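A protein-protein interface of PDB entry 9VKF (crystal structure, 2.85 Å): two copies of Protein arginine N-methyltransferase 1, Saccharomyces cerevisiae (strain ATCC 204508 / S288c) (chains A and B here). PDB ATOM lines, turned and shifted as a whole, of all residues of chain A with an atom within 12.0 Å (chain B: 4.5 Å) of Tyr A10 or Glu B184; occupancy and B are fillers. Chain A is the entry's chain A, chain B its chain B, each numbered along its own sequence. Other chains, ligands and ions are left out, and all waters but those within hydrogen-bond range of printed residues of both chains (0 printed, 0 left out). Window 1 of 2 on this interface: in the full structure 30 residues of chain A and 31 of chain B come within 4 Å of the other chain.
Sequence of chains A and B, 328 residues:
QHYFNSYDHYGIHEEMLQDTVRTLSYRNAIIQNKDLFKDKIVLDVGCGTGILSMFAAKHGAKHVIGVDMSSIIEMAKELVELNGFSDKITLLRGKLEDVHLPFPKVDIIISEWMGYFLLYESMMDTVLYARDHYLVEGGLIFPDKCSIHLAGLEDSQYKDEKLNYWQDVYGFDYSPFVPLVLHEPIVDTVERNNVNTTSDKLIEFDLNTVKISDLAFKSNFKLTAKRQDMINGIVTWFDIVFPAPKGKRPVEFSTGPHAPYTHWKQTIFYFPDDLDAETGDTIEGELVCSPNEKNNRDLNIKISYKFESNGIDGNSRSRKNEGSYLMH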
ATOM      1  N   TYR A  10      22.890 -14.071  22.757  1.00  0.00           N
ATOM      2  CA  TYR A  10      22.211 -13.317  23.803  1.00  0.00           C
ATOM      3  C   TYR A  10      22.898 -13.504  25.157  1.00  0.00           C
ATOM      4  O   TYR A  10      22.920 -12.591  25.983  1.00  0.00           O
ATOM      5  CB  TYR A  10      20.739 -13.736  23.874  1.00  0.00           C
ATOM      6  CG  TYR A  10      20.130 -13.681  25.257  1.00  0.00           C
ATOM      7  CD1 TYR A  10      19.830 -12.468  25.857  1.00  0.00           C
ATOM      8  CD2 TYR A  10      19.843 -14.846  25.956  1.00  0.00           C
ATOM      9  CE1 TYR A  10      19.274 -12.413  27.118  1.00  0.00           C
ATOM     10  CE2 TYR A  10      19.283 -14.802  27.218  1.00  0.00           C
ATOM     11  CZ  TYR A  10      19.002 -13.582  27.793  1.00  0.00           C
ATOM     12  OH  TYR A  10      18.445 -13.526  29.050  1.00  0.00           O
ATOM     13  N   GLY A  11      23.445 -14.686  25.403  1.00  0.00           N
ATOM     14  CA  GLY A  11      24.140 -14.913  26.651  1.00  0.00           C
ATOM     15  C   GLY A  11      25.206 -13.863  26.867  1.00  0.00           C
ATOM     16  O   GLY A  11      25.154 -13.114  27.840  1.00  0.00           O
ATOM     17  N   ILE A  12      26.162 -13.777  25.951  1.00  0.00           N
ATOM     18  CA  ILE A  12      27.265 -12.843  26.122  1.00  0.00           C
ATOM     19  C   ILE A  12      26.798 -11.430  26.372  1.00  0.00           C
ATOM     20  O   ILE A  12      27.271 -10.786  27.293  1.00  0.00           O
ATOM     21  CB  ILE A  12      28.153 -12.797  24.875  1.00  0.00           C
ATOM     22  CG1 ILE A  12      28.878 -14.125  24.711  1.00  0.00           C
ATOM     23  CG2 ILE A  12      29.144 -11.651  24.977  1.00  0.00           C
ATOM     24  CD1 ILE A  12      28.371 -14.926  23.540  1.00  0.00           C
ATOM     25  N   HIS A  13      25.864 -10.939  25.569  1.00  0.00           N
ATOM     26  CA  HIS A  13      25.474  -9.539  25.711  1.00  0.00           C
ATOM     27  C   HIS A  13      24.861  -9.262  27.077  1.00  0.00           C
ATOM     28  O   HIS A  13      25.111  -8.205  27.672  1.00  0.00           O
ATOM     29  CB  HIS A  13      24.510  -9.149  24.592  1.00  0.00           C
ATOM     30  CG  HIS A  13      25.179  -8.949  23.268  1.00  0.00           C
ATOM     31  ND1 HIS A  13      26.177  -8.021  23.075  1.00  0.00           N
ATOM     32  CD2 HIS A  13      24.999  -9.563  22.075  1.00  0.00           C
ATOM     33  CE1 HIS A  13      26.582  -8.066  21.819  1.00  0.00           C
ATOM     34  NE2 HIS A  13      25.883  -8.994  21.191  1.00  0.00           N
ATOM     35  N   GLU A  14      24.051 -10.192  27.590  1.00  0.00           N
ATOM     36  CA  GLU A  14      23.533 -10.044  28.945  1.00  0.00           C
ATOM     37  C   GLU A  14      24.667 -10.053  29.962  1.00  0.00           C
ATOM     38  O   GLU A  14      24.642  -9.294  30.939  1.00  0.00           O
ATOM     39  CB  GLU A  14      22.522 -11.152  29.240  1.00  0.00           C
ATOM     40  CG  GLU A  14      22.032 -11.191  30.680  1.00  0.00           C
ATOM     41  CD  GLU A  14      21.418 -12.528  31.049  1.00  0.00           C
ATOM     42  OE1 GLU A  14      22.126 -13.552  30.965  1.00  0.00           O
ATOM     43  OE2 GLU A  14      20.227 -12.554  31.421  1.00  0.00           O
ATOM     44  N   GLU A  15      25.675 -10.902  29.744  1.00  0.00           N
ATOM     45  CA  GLU A  15      26.821 -10.955  30.646  1.00  0.00           C
ATOM     46  C   GLU A  15      27.586  -9.636  30.651  1.00  0.00           C
ATOM     47  O   GLU A  15      28.027  -9.170  31.709  1.00  0.00           O
ATOM     48  CB  GLU A  15      27.735 -12.114  30.250  1.00  0.00           C
ATOM     49  CG  GLU A  15      29.022 -12.191  31.043  1.00  0.00           C
ATOM     50  CD  GLU A  15      29.835 -13.430  30.727  1.00  0.00           C
ATOM     51  OE1 GLU A  15      30.472 -13.471  29.653  1.00  0.00           O
ATOM     52  OE2 GLU A  15      29.841 -14.361  31.557  1.00  0.00           O
ATOM     53  N   MET A  16      27.762  -9.027  29.475  1.00  0.00           N
ATOM     54  CA  MET A  16      28.422  -7.727  29.394  1.00  0.00           C
ATOM     55  C   MET A  16      27.682  -6.683  30.221  1.00  0.00           C
ATOM     56  O   MET A  16      28.269  -6.031  31.092  1.00  0.00           O
ATOM     57  CB  MET A  16      28.516  -7.279  27.935  1.00  0.00           C
ATOM     58  CG  MET A  16      29.379  -8.166  27.059  1.00  0.00           C
ATOM     59  SD  MET A  16      31.048  -8.416  27.680  1.00  0.00           S
ATOM     60  CE  MET A  16      31.946  -7.376  26.543  1.00  0.00           C
ATOM     61  N   LEU A  17      26.381  -6.519  29.962  1.00  0.00           N
ATOM     62  CA  LEU A  17      25.618  -5.453  30.600  1.00  0.00           C
ATOM     63  C   LEU A  17      25.488  -5.662  32.105  1.00  0.00           C
ATOM     64  O   LEU A  17      25.462  -4.686  32.862  1.00  0.00           O
ATOM     65  CB  LEU A  17      24.240  -5.350  29.952  1.00  0.00           C
ATOM     66  CG  LEU A  17      24.276  -4.988  28.466  1.00  0.00           C
ATOM     67  CD1 LEU A  17      22.933  -5.244  27.802  1.00  0.00           C
ATOM     68  CD2 LEU A  17      24.712  -3.544  28.272  1.00  0.00           C
ATOM     69  N   GLN A  18      25.394  -6.914  32.557  1.00  0.00           N
ATOM     70  CA  GLN A  18      25.288  -7.186  33.985  1.00  0.00           C
ATOM     71  C   GLN A  18      26.619  -7.066  34.714  1.00  0.00           C
ATOM     72  O   GLN A  18      26.632  -7.092  35.950  1.00  0.00           O
ATOM     73  CB  GLN A  18      24.690  -8.576  34.224  1.00  0.00           C
ATOM     74  CG  GLN A  18      23.260  -8.723  33.729  1.00  0.00           C
ATOM     75  CD  GLN A  18      22.500  -9.823  34.446  1.00  0.00           C
ATOM     76  OE1 GLN A  18      22.710 -11.009  34.189  1.00  0.00           O
ATOM     77  NE2 GLN A  18      21.617  -9.433  35.358  1.00  0.00           N
ATOM     78  N   ASP A  19      27.730  -6.940  33.992  1.00  0.00           N
ATOM     79  CA  ASP A  19      29.011  -6.612  34.612  1.00  0.00           C
ATOM     80  C   ASP A  19      28.990  -5.116  34.900  1.00  0.00           C
ATOM     81  O   ASP A  19      29.380  -4.291  34.072  1.00  0.00           O
ATOM     82  CB  ASP A  19      30.174  -7.004  33.707  1.00  0.00           C
ATOM     83  CG  ASP A  19      31.514  -6.982  34.427  1.00  0.00           C
ATOM     84  OD1 ASP A  19      31.662  -6.219  35.406  1.00  0.00           O
ATOM     85  OD2 ASP A  19      32.425  -7.734  34.015  1.00  0.00           O
ATOM     86  N   ARG A  22      32.512  -3.159  34.856  1.00  0.00           N
ATOM     87  CA  ARG A  22      32.943  -2.724  33.562  1.00  0.00           C
ATOM     88  C   ARG A  22      32.081  -1.651  32.990  1.00  0.00           C
ATOM     89  O   ARG A  22      32.579  -0.610  32.658  1.00  0.00           O
ATOM     90  CB  ARG A  22      32.900  -3.903  32.615  1.00  0.00           C
ATOM     91  CG  ARG A  22      33.346  -3.636  31.196  1.00  0.00           C
ATOM     92  CD  ARG A  22      32.664  -4.584  30.228  1.00  0.00           C
ATOM     93  NE  ARG A  22      31.275  -4.193  30.023  1.00  0.00           N
ATOM     94  CZ  ARG A  22      30.777  -3.662  28.913  1.00  0.00           C
ATOM     95  NH1 ARG A  22      31.534  -3.421  27.856  1.00  0.00           N
ATOM     96  NH2 ARG A  22      29.494  -3.357  28.862  1.00  0.00           N
ATOM     97  N   GLY A  48      28.794  -3.900  19.964  1.00  0.00           N
ATOM     98  CA  GLY A  48      27.832  -4.844  20.512  1.00  0.00           C
ATOM     99  C   GLY A  48      26.413  -4.328  20.369  1.00  0.00           C
ATOM    100  O   GLY A  48      25.935  -4.049  19.262  1.00  0.00           O
ATOM    101  N   THR A  49      25.719  -4.194  21.499  1.00  0.00           N
ATOM    102  CA  THR A  49      24.377  -3.629  21.500  1.00  0.00           C
ATOM    103  C   THR A  49      24.374  -2.116  21.331  1.00  0.00           C
ATOM    104  O   THR A  49      23.305  -1.535  21.114  1.00  0.00           O
ATOM    105  CB  THR A  49      23.650  -3.996  22.796  1.00  0.00           C
ATOM    106  OG1 THR A  49      24.391  -3.502  23.921  1.00  0.00           O
ATOM    107  CG2 THR A  49      23.505  -5.505  22.916  1.00  0.00           C
ATOM    108  N   ASP A  68      30.407  -3.476  14.530  1.00  0.00           N
ATOM    109  CA  ASP A  68      30.472  -4.834  15.054  1.00  0.00           C
ATOM    110  C   ASP A  68      30.123  -5.768  13.906  1.00  0.00           C
ATOM    111  O   ASP A  68      29.150  -5.544  13.212  1.00  0.00           O
ATOM    112  CB  ASP A  68      29.514  -5.056  16.209  1.00  0.00           C
ATOM    113  CG  ASP A  68      29.916  -6.226  17.072  1.00  0.00           C
ATOM    114  OD1 ASP A  68      30.647  -7.110  16.588  1.00  0.00           O
ATOM    115  OD2 ASP A  68      29.508  -6.263  18.244  1.00  0.00           O
ATOM    116  N   SER A  70      28.942  -8.690  14.070  1.00  0.00           N
ATOM    117  CA  SER A  70      27.895  -9.627  14.446  1.00  0.00           C
ATOM    118  C   SER A  70      26.544  -9.144  13.934  1.00  0.00           C
ATOM    119  O   SER A  70      26.367  -7.977  13.577  1.00  0.00           O
ATOM    120  CB  SER A  70      27.846  -9.803  15.964  1.00  0.00           C
ATOM    121  OG  SER A  70      29.036 -10.399  16.448  1.00  0.00           O
ATOM    122  N   SER A  71      25.583 -10.070  13.896  1.00  0.00           N
ATOM    123  CA  SER A  71      24.221  -9.719  13.512  1.00  0.00           C
ATOM    124  C   SER A  71      23.527  -8.856  14.555  1.00  0.00           C
ATOM    125  O   SER A  71      22.422  -8.366  14.293  1.00  0.00           O
ATOM    126  CB  SER A  71      23.400 -10.984  13.261  1.00  0.00           C
ATOM    127  OG  SER A  71      23.283 -11.758  14.441  1.00  0.00           O
ATOM    128  N   ILE A  72      24.191  -8.583  15.673  1.00  0.00           N
ATOM    129  CA  ILE A  72      23.647  -7.721  16.724  1.00  0.00           C
ATOM    130  C   ILE A  72      23.450  -6.282  16.297  1.00  0.00           C
ATOM    131  O   ILE A  72      22.626  -5.580  16.872  1.00  0.00           O
ATOM    132  CB  ILE A  72      24.598  -7.728  17.941  1.00  0.00           C
ATOM    133  CG1 ILE A  72      23.963  -7.116  19.188  1.00  0.00           C
ATOM    134  CG2 ILE A  72      25.873  -6.971  17.615  1.00  0.00           C
ATOM    135  CD1 ILE A  72      22.949  -8.012  19.853  1.00  0.00           C
ATOM    136  N   ILE A  73      24.189  -5.817  15.293  1.00  0.00           N
ATOM    137  CA  ILE A  73      24.112  -4.412  14.886  1.00  0.00           C
ATOM    138  C   ILE A  73      22.689  -4.063  14.590  1.00  0.00           C
ATOM    139  O   ILE A  73      22.286  -2.917  14.661  1.00  0.00           O
ATOM    140  CB  ILE A  73      25.001  -4.126  13.669  1.00  0.00           C
ATOM    141  CG1 ILE A  73      26.447  -3.872  14.109  1.00  0.00           C
ATOM    142  CG2 ILE A  73      24.483  -2.943  12.862  1.00  0.00           C
ATOM    143  CD1 ILE A  73      26.798  -2.421  14.353  1.00  0.00           C
ATOM    144  N   MET A  75      19.967  -4.987  16.411  1.00  0.00           N
ATOM    145  CA  MET A  75      19.271  -4.596  17.629  1.00  0.00           C
ATOM    146  C   MET A  75      19.827  -3.282  18.088  1.00  0.00           C
ATOM    147  O   MET A  75      19.116  -2.479  18.593  1.00  0.00           O
ATOM    148  CB  MET A  75      19.455  -5.633  18.716  1.00  0.00           C
ATOM    149  CG  MET A  75      18.755  -5.283  20.011  1.00  0.00           C
ATOM    150  SD  MET A  75      17.080  -5.893  20.072  1.00  0.00           S
ATOM    151  CE  MET A  75      17.417  -7.572  20.545  1.00  0.00           C
ATOM    152  N   ALA A  76      21.107  -3.076  17.928  1.00  0.00           N
ATOM    153  CA  ALA A  76      21.721  -1.842  18.264  1.00  0.00           C
ATOM    154  C   ALA A  76      20.928  -0.771  17.622  1.00  0.00           C
ATOM    155  O   ALA A  76      20.613   0.229  18.241  1.00  0.00           O
ATOM    156  CB  ALA A  76      23.122  -1.826  17.732  1.00  0.00           C
ATOM    157  N   LEU A  79      17.536  -0.413  19.259  1.00  0.00           N
ATOM    158  CA  LEU A  79      17.630   0.202  20.561  1.00  0.00           C
ATOM    159  C   LEU A  79      17.977   1.653  20.373  1.00  0.00           C
ATOM    160  O   LEU A  79      17.338   2.500  20.946  1.00  0.00           O
ATOM    161  CB  LEU A  79      18.666  -0.530  21.391  1.00  0.00           C
ATOM    162  CG  LEU A  79      18.378  -1.988  21.712  1.00  0.00           C
ATOM    163  CD1 LEU A  79      19.681  -2.694  22.016  1.00  0.00           C
ATOM    164  CD2 LEU A  79      17.425  -2.109  22.882  1.00  0.00           C
ATOM    165  N   HIS A 263      32.868 -10.034  34.905  1.00  0.00           N
ATOM    166  CA  HIS A 263      32.596 -11.176  34.043  1.00  0.00           C
ATOM    167  C   HIS A 263      33.865 -11.800  33.482  1.00  0.00           C
ATOM    168  O   HIS A 263      33.783 -12.844  32.823  1.00  0.00           O
ATOM    169  CB  HIS A 263      31.657 -10.767  32.907  1.00  0.00           C
ATOM    170  CG  HIS A 263      32.355 -10.224  31.699  1.00  0.00           C
ATOM    171  ND1 HIS A 263      32.657  -8.887  31.552  1.00  0.00           N
ATOM    172  CD2 HIS A 263      32.796 -10.835  30.574  1.00  0.00           C
ATOM    173  CE1 HIS A 263      33.261  -8.699  30.392  1.00  0.00           C
ATOM    174  NE2 HIS A 263      33.359  -9.865  29.780  1.00  0.00           N
ATOM    175  N   TRP B 166      15.419  -6.166  31.048  1.00  0.00           N
ATOM    176  CA  TRP B 166      15.582  -5.351  29.855  1.00  0.00           C
ATOM    177  C   TRP B 166      14.661  -4.139  29.826  1.00  0.00           C
ATOM    178  O   TRP B 166      14.723  -3.352  28.877  1.00  0.00           O
ATOM    179  CB  TRP B 166      15.357  -6.213  28.613  1.00  0.00           C
ATOM    180  CG  TRP B 166      16.208  -7.441  28.625  1.00  0.00           C
ATOM    181  CD1 TRP B 166      15.806  -8.717  28.902  1.00  0.00           C
ATOM    182  CD2 TRP B 166      17.618  -7.507  28.387  1.00  0.00           C
ATOM    183  NE1 TRP B 166      16.877  -9.575  28.832  1.00  0.00           N
ATOM    184  CE2 TRP B 166      18.001  -8.856  28.519  1.00  0.00           C
ATOM    185  CE3 TRP B 166      18.592  -6.557  28.065  1.00  0.00           C
ATOM    186  CZ2 TRP B 166      19.317  -9.279  28.342  1.00  0.00           C
ATOM    187  CZ3 TRP B 166      19.896  -6.978  27.890  1.00  0.00           C
ATOM    188  CH2 TRP B 166      20.247  -8.327  28.028  1.00  0.00           C
ATOM    189  N   PHE B 177      14.841  -6.287  23.335  1.00  0.00           N
ATOM    190  CA  PHE B 177      15.636  -7.481  23.584  1.00  0.00           C
ATOM    191  C   PHE B 177      14.783  -8.629  24.077  1.00  0.00           C
ATOM    192  O   PHE B 177      15.174  -9.774  23.984  1.00  0.00           O
ATOM    193  CB  PHE B 177      16.704  -7.175  24.630  1.00  0.00           C
ATOM    194  CG  PHE B 177      18.026  -7.825  24.377  1.00  0.00           C
ATOM    195  CD1 PHE B 177      18.158  -9.196  24.386  1.00  0.00           C
ATOM    196  CD2 PHE B 177      19.145  -7.055  24.154  1.00  0.00           C
ATOM    197  CE1 PHE B 177      19.379  -9.788  24.157  1.00  0.00           C
ATOM    198  CE2 PHE B 177      20.367  -7.640  23.926  1.00  0.00           C
ATOM    199  CZ  PHE B 177      20.487  -9.010  23.928  1.00  0.00           C
ATOM    200  N   LEU B 180      14.261 -11.726  22.056  1.00  0.00           N
ATOM    201  CA  LEU B 180      15.403 -12.599  21.965  1.00  0.00           C
ATOM    202  C   LEU B 180      15.405 -13.612  23.084  1.00  0.00           C
ATOM    203  O   LEU B 180      15.783 -14.758  22.892  1.00  0.00           O
ATOM    204  CB  LEU B 180      16.693 -11.810  22.033  1.00  0.00           C
ATOM    205  CG  LEU B 180      17.251 -11.237  20.745  1.00  0.00           C
ATOM    206  CD1 LEU B 180      18.423 -10.360  21.105  1.00  0.00           C
ATOM    207  CD2 LEU B 180      17.706 -12.338  19.813  1.00  0.00           C
ATOM    208  N   VAL B 181      14.990 -13.193  24.263  1.00  0.00           N
ATOM    209  CA  VAL B 181      15.018 -14.108  25.400  1.00  0.00           C
ATOM    210  C   VAL B 181      13.965 -15.197  25.235  1.00  0.00           C
ATOM    211  O   VAL B 181      14.202 -16.365  25.566  1.00  0.00           O
ATOM    212  CB  VAL B 181      14.828 -13.331  26.715  1.00  0.00           C
ATOM    213  CG1 VAL B 181      15.002 -14.253  27.914  1.00  0.00           C
ATOM    214  CG2 VAL B 181      15.797 -12.164  26.784  1.00  0.00           C
ATOM    215  N   LEU B 182      12.785 -14.833  24.727  1.00  0.00           N
ATOM    216  CA  LEU B 182      11.734 -15.820  24.511  1.00  0.00           C
ATOM    217  C   LEU B 182      12.111 -16.823  23.428  1.00  0.00           C
ATOM    218  O   LEU B 182      11.623 -17.958  23.444  1.00  0.00           O
ATOM    219  CB  LEU B 182      10.420 -15.124  24.157  1.00  0.00           C
ATOM    220  CG  LEU B 182       9.750 -14.321  25.273  1.00  0.00           C
ATOM    221  CD1 LEU B 182       8.536 -13.575  24.744  1.00  0.00           C
ATOM    222  CD2 LEU B 182       9.357 -15.231  26.426  1.00  0.00           C
ATOM    223  N   HIS B 183      12.973 -16.432  22.487  1.00  0.00           N
ATOM    224  CA  HIS B 183      13.311 -17.298  21.366  1.00  0.00           C
ATOM    225  C   HIS B 183      14.459 -18.252  21.661  1.00  0.00           C
ATOM    226  O   HIS B 183      14.583 -19.276  20.980  1.00  0.00           O
ATOM    227  CB  HIS B 183      13.695 -16.462  20.140  1.00  0.00           C
ATOM    228  CG  HIS B 183      12.585 -15.612  19.605  1.00  0.00           C
ATOM    229  ND1 HIS B 183      12.773 -14.703  18.586  1.00  0.00           N
ATOM    230  CD2 HIS B 183      11.278 -15.525  19.949  1.00  0.00           C
ATOM    231  CE1 HIS B 183      11.630 -14.095  18.323  1.00  0.00           C
ATOM    232  NE2 HIS B 183      10.707 -14.576  19.136  1.00  0.00           N
ATOM    233  N   GLU B 184      15.294 -17.951  22.646  1.00  0.00           N
ATOM    234  CA  GLU B 184      16.443 -18.826  22.845  1.00  0.00           C
ATOM    235  C   GLU B 184      16.060 -20.012  23.723  1.00  0.00           C
ATOM    236  O   GLU B 184      15.544 -19.813  24.829  1.00  0.00           O
ATOM    237  CB  GLU B 184      17.603 -18.074  23.481  1.00  0.00           C
ATOM    238  CG  GLU B 184      18.965 -18.674  23.156  1.00  0.00           C
ATOM    239  CD  GLU B 184      19.950 -18.550  24.300  1.00  0.00           C
ATOM    240  OE1 GLU B 184      19.578 -18.881  25.443  1.00  0.00           O
ATOM    241  OE2 GLU B 184      21.095 -18.121  24.056  1.00  0.00           O
ATOM    242  N   PRO B 185      16.293 -21.241  23.273  1.00  0.00           N
ATOM    243  CA  PRO B 185      16.052 -22.399  24.138  1.00  0.00           C
ATOM    244  C   PRO B 185      17.079 -22.468  25.257  1.00  0.00           C
ATOM    245  O   PRO B 185      18.216 -22.009  25.123  1.00  0.00           O
ATOM    246  CB  PRO B 185      16.184 -23.590  23.184  1.00  0.00           C
ATOM    247  CG  PRO B 185      17.084 -23.091  22.108  1.00  0.00           C
ATOM    248  CD  PRO B 185      16.755 -21.637  21.933  1.00  0.00           C
ATOM    249  N   ILE B 186      16.662 -23.051  26.376  1.00  0.00           N
ATOM    250  CA  ILE B 186      17.474 -23.110  27.586  1.00  0.00           C
ATOM    251  C   ILE B 186      17.755 -24.566  27.917  1.00  0.00           C
ATOM    252  O   ILE B 186      16.823 -25.355  28.116  1.00  0.00           O
ATOM    253  CB  ILE B 186      16.788 -22.406  28.763  1.00  0.00           C
ATOM    254  CG1 ILE B 186      16.287 -21.032  28.321  1.00  0.00           C
ATOM    255  CG2 ILE B 186      17.741 -22.289  29.945  1.00  0.00           C
ATOM    256  CD1 ILE B 186      15.380 -20.385  29.306  1.00  0.00           C
ATOM    257  N   HIS B 328      21.598 -22.150  17.777  1.00  0.00           N
ATOM    258  CA  HIS B 328      22.744 -21.672  17.014  1.00  0.00           C
ATOM    259  C   HIS B 328      24.053 -21.890  17.769  1.00  0.00           C
ATOM    260  O   HIS B 328      25.134 -21.902  17.182  1.00  0.00           O
ATOM    261  CB  HIS B 328      22.574 -20.187  16.701  1.00  0.00           C
ATOM    262  CG  HIS B 328      22.159 -19.374  17.887  1.00  0.00           C
ATOM    263  ND1 HIS B 328      22.959 -19.221  18.999  1.00  0.00           N
ATOM    264  CD2 HIS B 328      21.019 -18.693  18.147  1.00  0.00           C
ATOM    265  CE1 HIS B 328      22.335 -18.468  19.888  1.00  0.00           C
ATOM    266  NE2 HIS B 328      21.155 -18.135  19.395  1.00  0.00           N
ATOM    267  OXT HIS B 328      24.057 -22.051  18.989  1.00  0.00           O
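OE2 of Glu A14 lies within hydrogen-bond range of OH of Tyr A10.
Among the printed residues, merely in contact across the chains: Tyr A10 with Trp B166 (3.4 Å), Tyr A10 with Phe B177 (3.2 Å), Tyr A10 with Val B181 (3.5 Å), Tyr A10 with Glu B184 (3.99 Å), Glu A14 with Trp B166 (3.8 Å), Leu A17 with Trp B166 (3.5 Å), Thr A49 with Phe B177 (3.9 Å), Met A75 with Phe B177 (3.5 Å) and Met A75 with Leu B180 (3.0 Å).
Of the printed residues of chain B, Tyr A10 touches Trp B166, Phe B177, Val B181 and Glu B184. Printed residues of chain A within 4 Å of Glu B184: Tyr A10. Leu B180 touches just one residue of chain A: Met A75 (3.0 Å). Val B181 touches one residue of chain A. His B183 touches none of the printed residues of chain A. Of the printed residues of chain B, Thr A49 touches Phe B177. Printed residues of chain B within 4 Å of Leu A17: Trp B166. Leu B182 touches none of the printed residues of chain A. Ile A12 touches none of the printed residues of chain B. The nearest printed residue of chain B that does not touch Tyr A10 is Leu B180 (4.8 Å). The nearest printed residue of chain B that does not touch Leu A17 is Phe B177 (5.2 Å).
Of the 10 printed residues of chain B, 5 touch a printed residue of chain A. Hydrophobic or aromatic side chains of chain B within 4 Å of the printed part of chain A: Trp B166, Phe B177, Leu B180 and Val B181. Along chain B the printed residues that touch a printed residue of chain A span positions 166 to 184. Among the printed residues, no Asp or Glu carboxylate lies within 4 Å of a Lys or Arg side-chain nitrogen of the other chain.
No position is printed for both chains.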
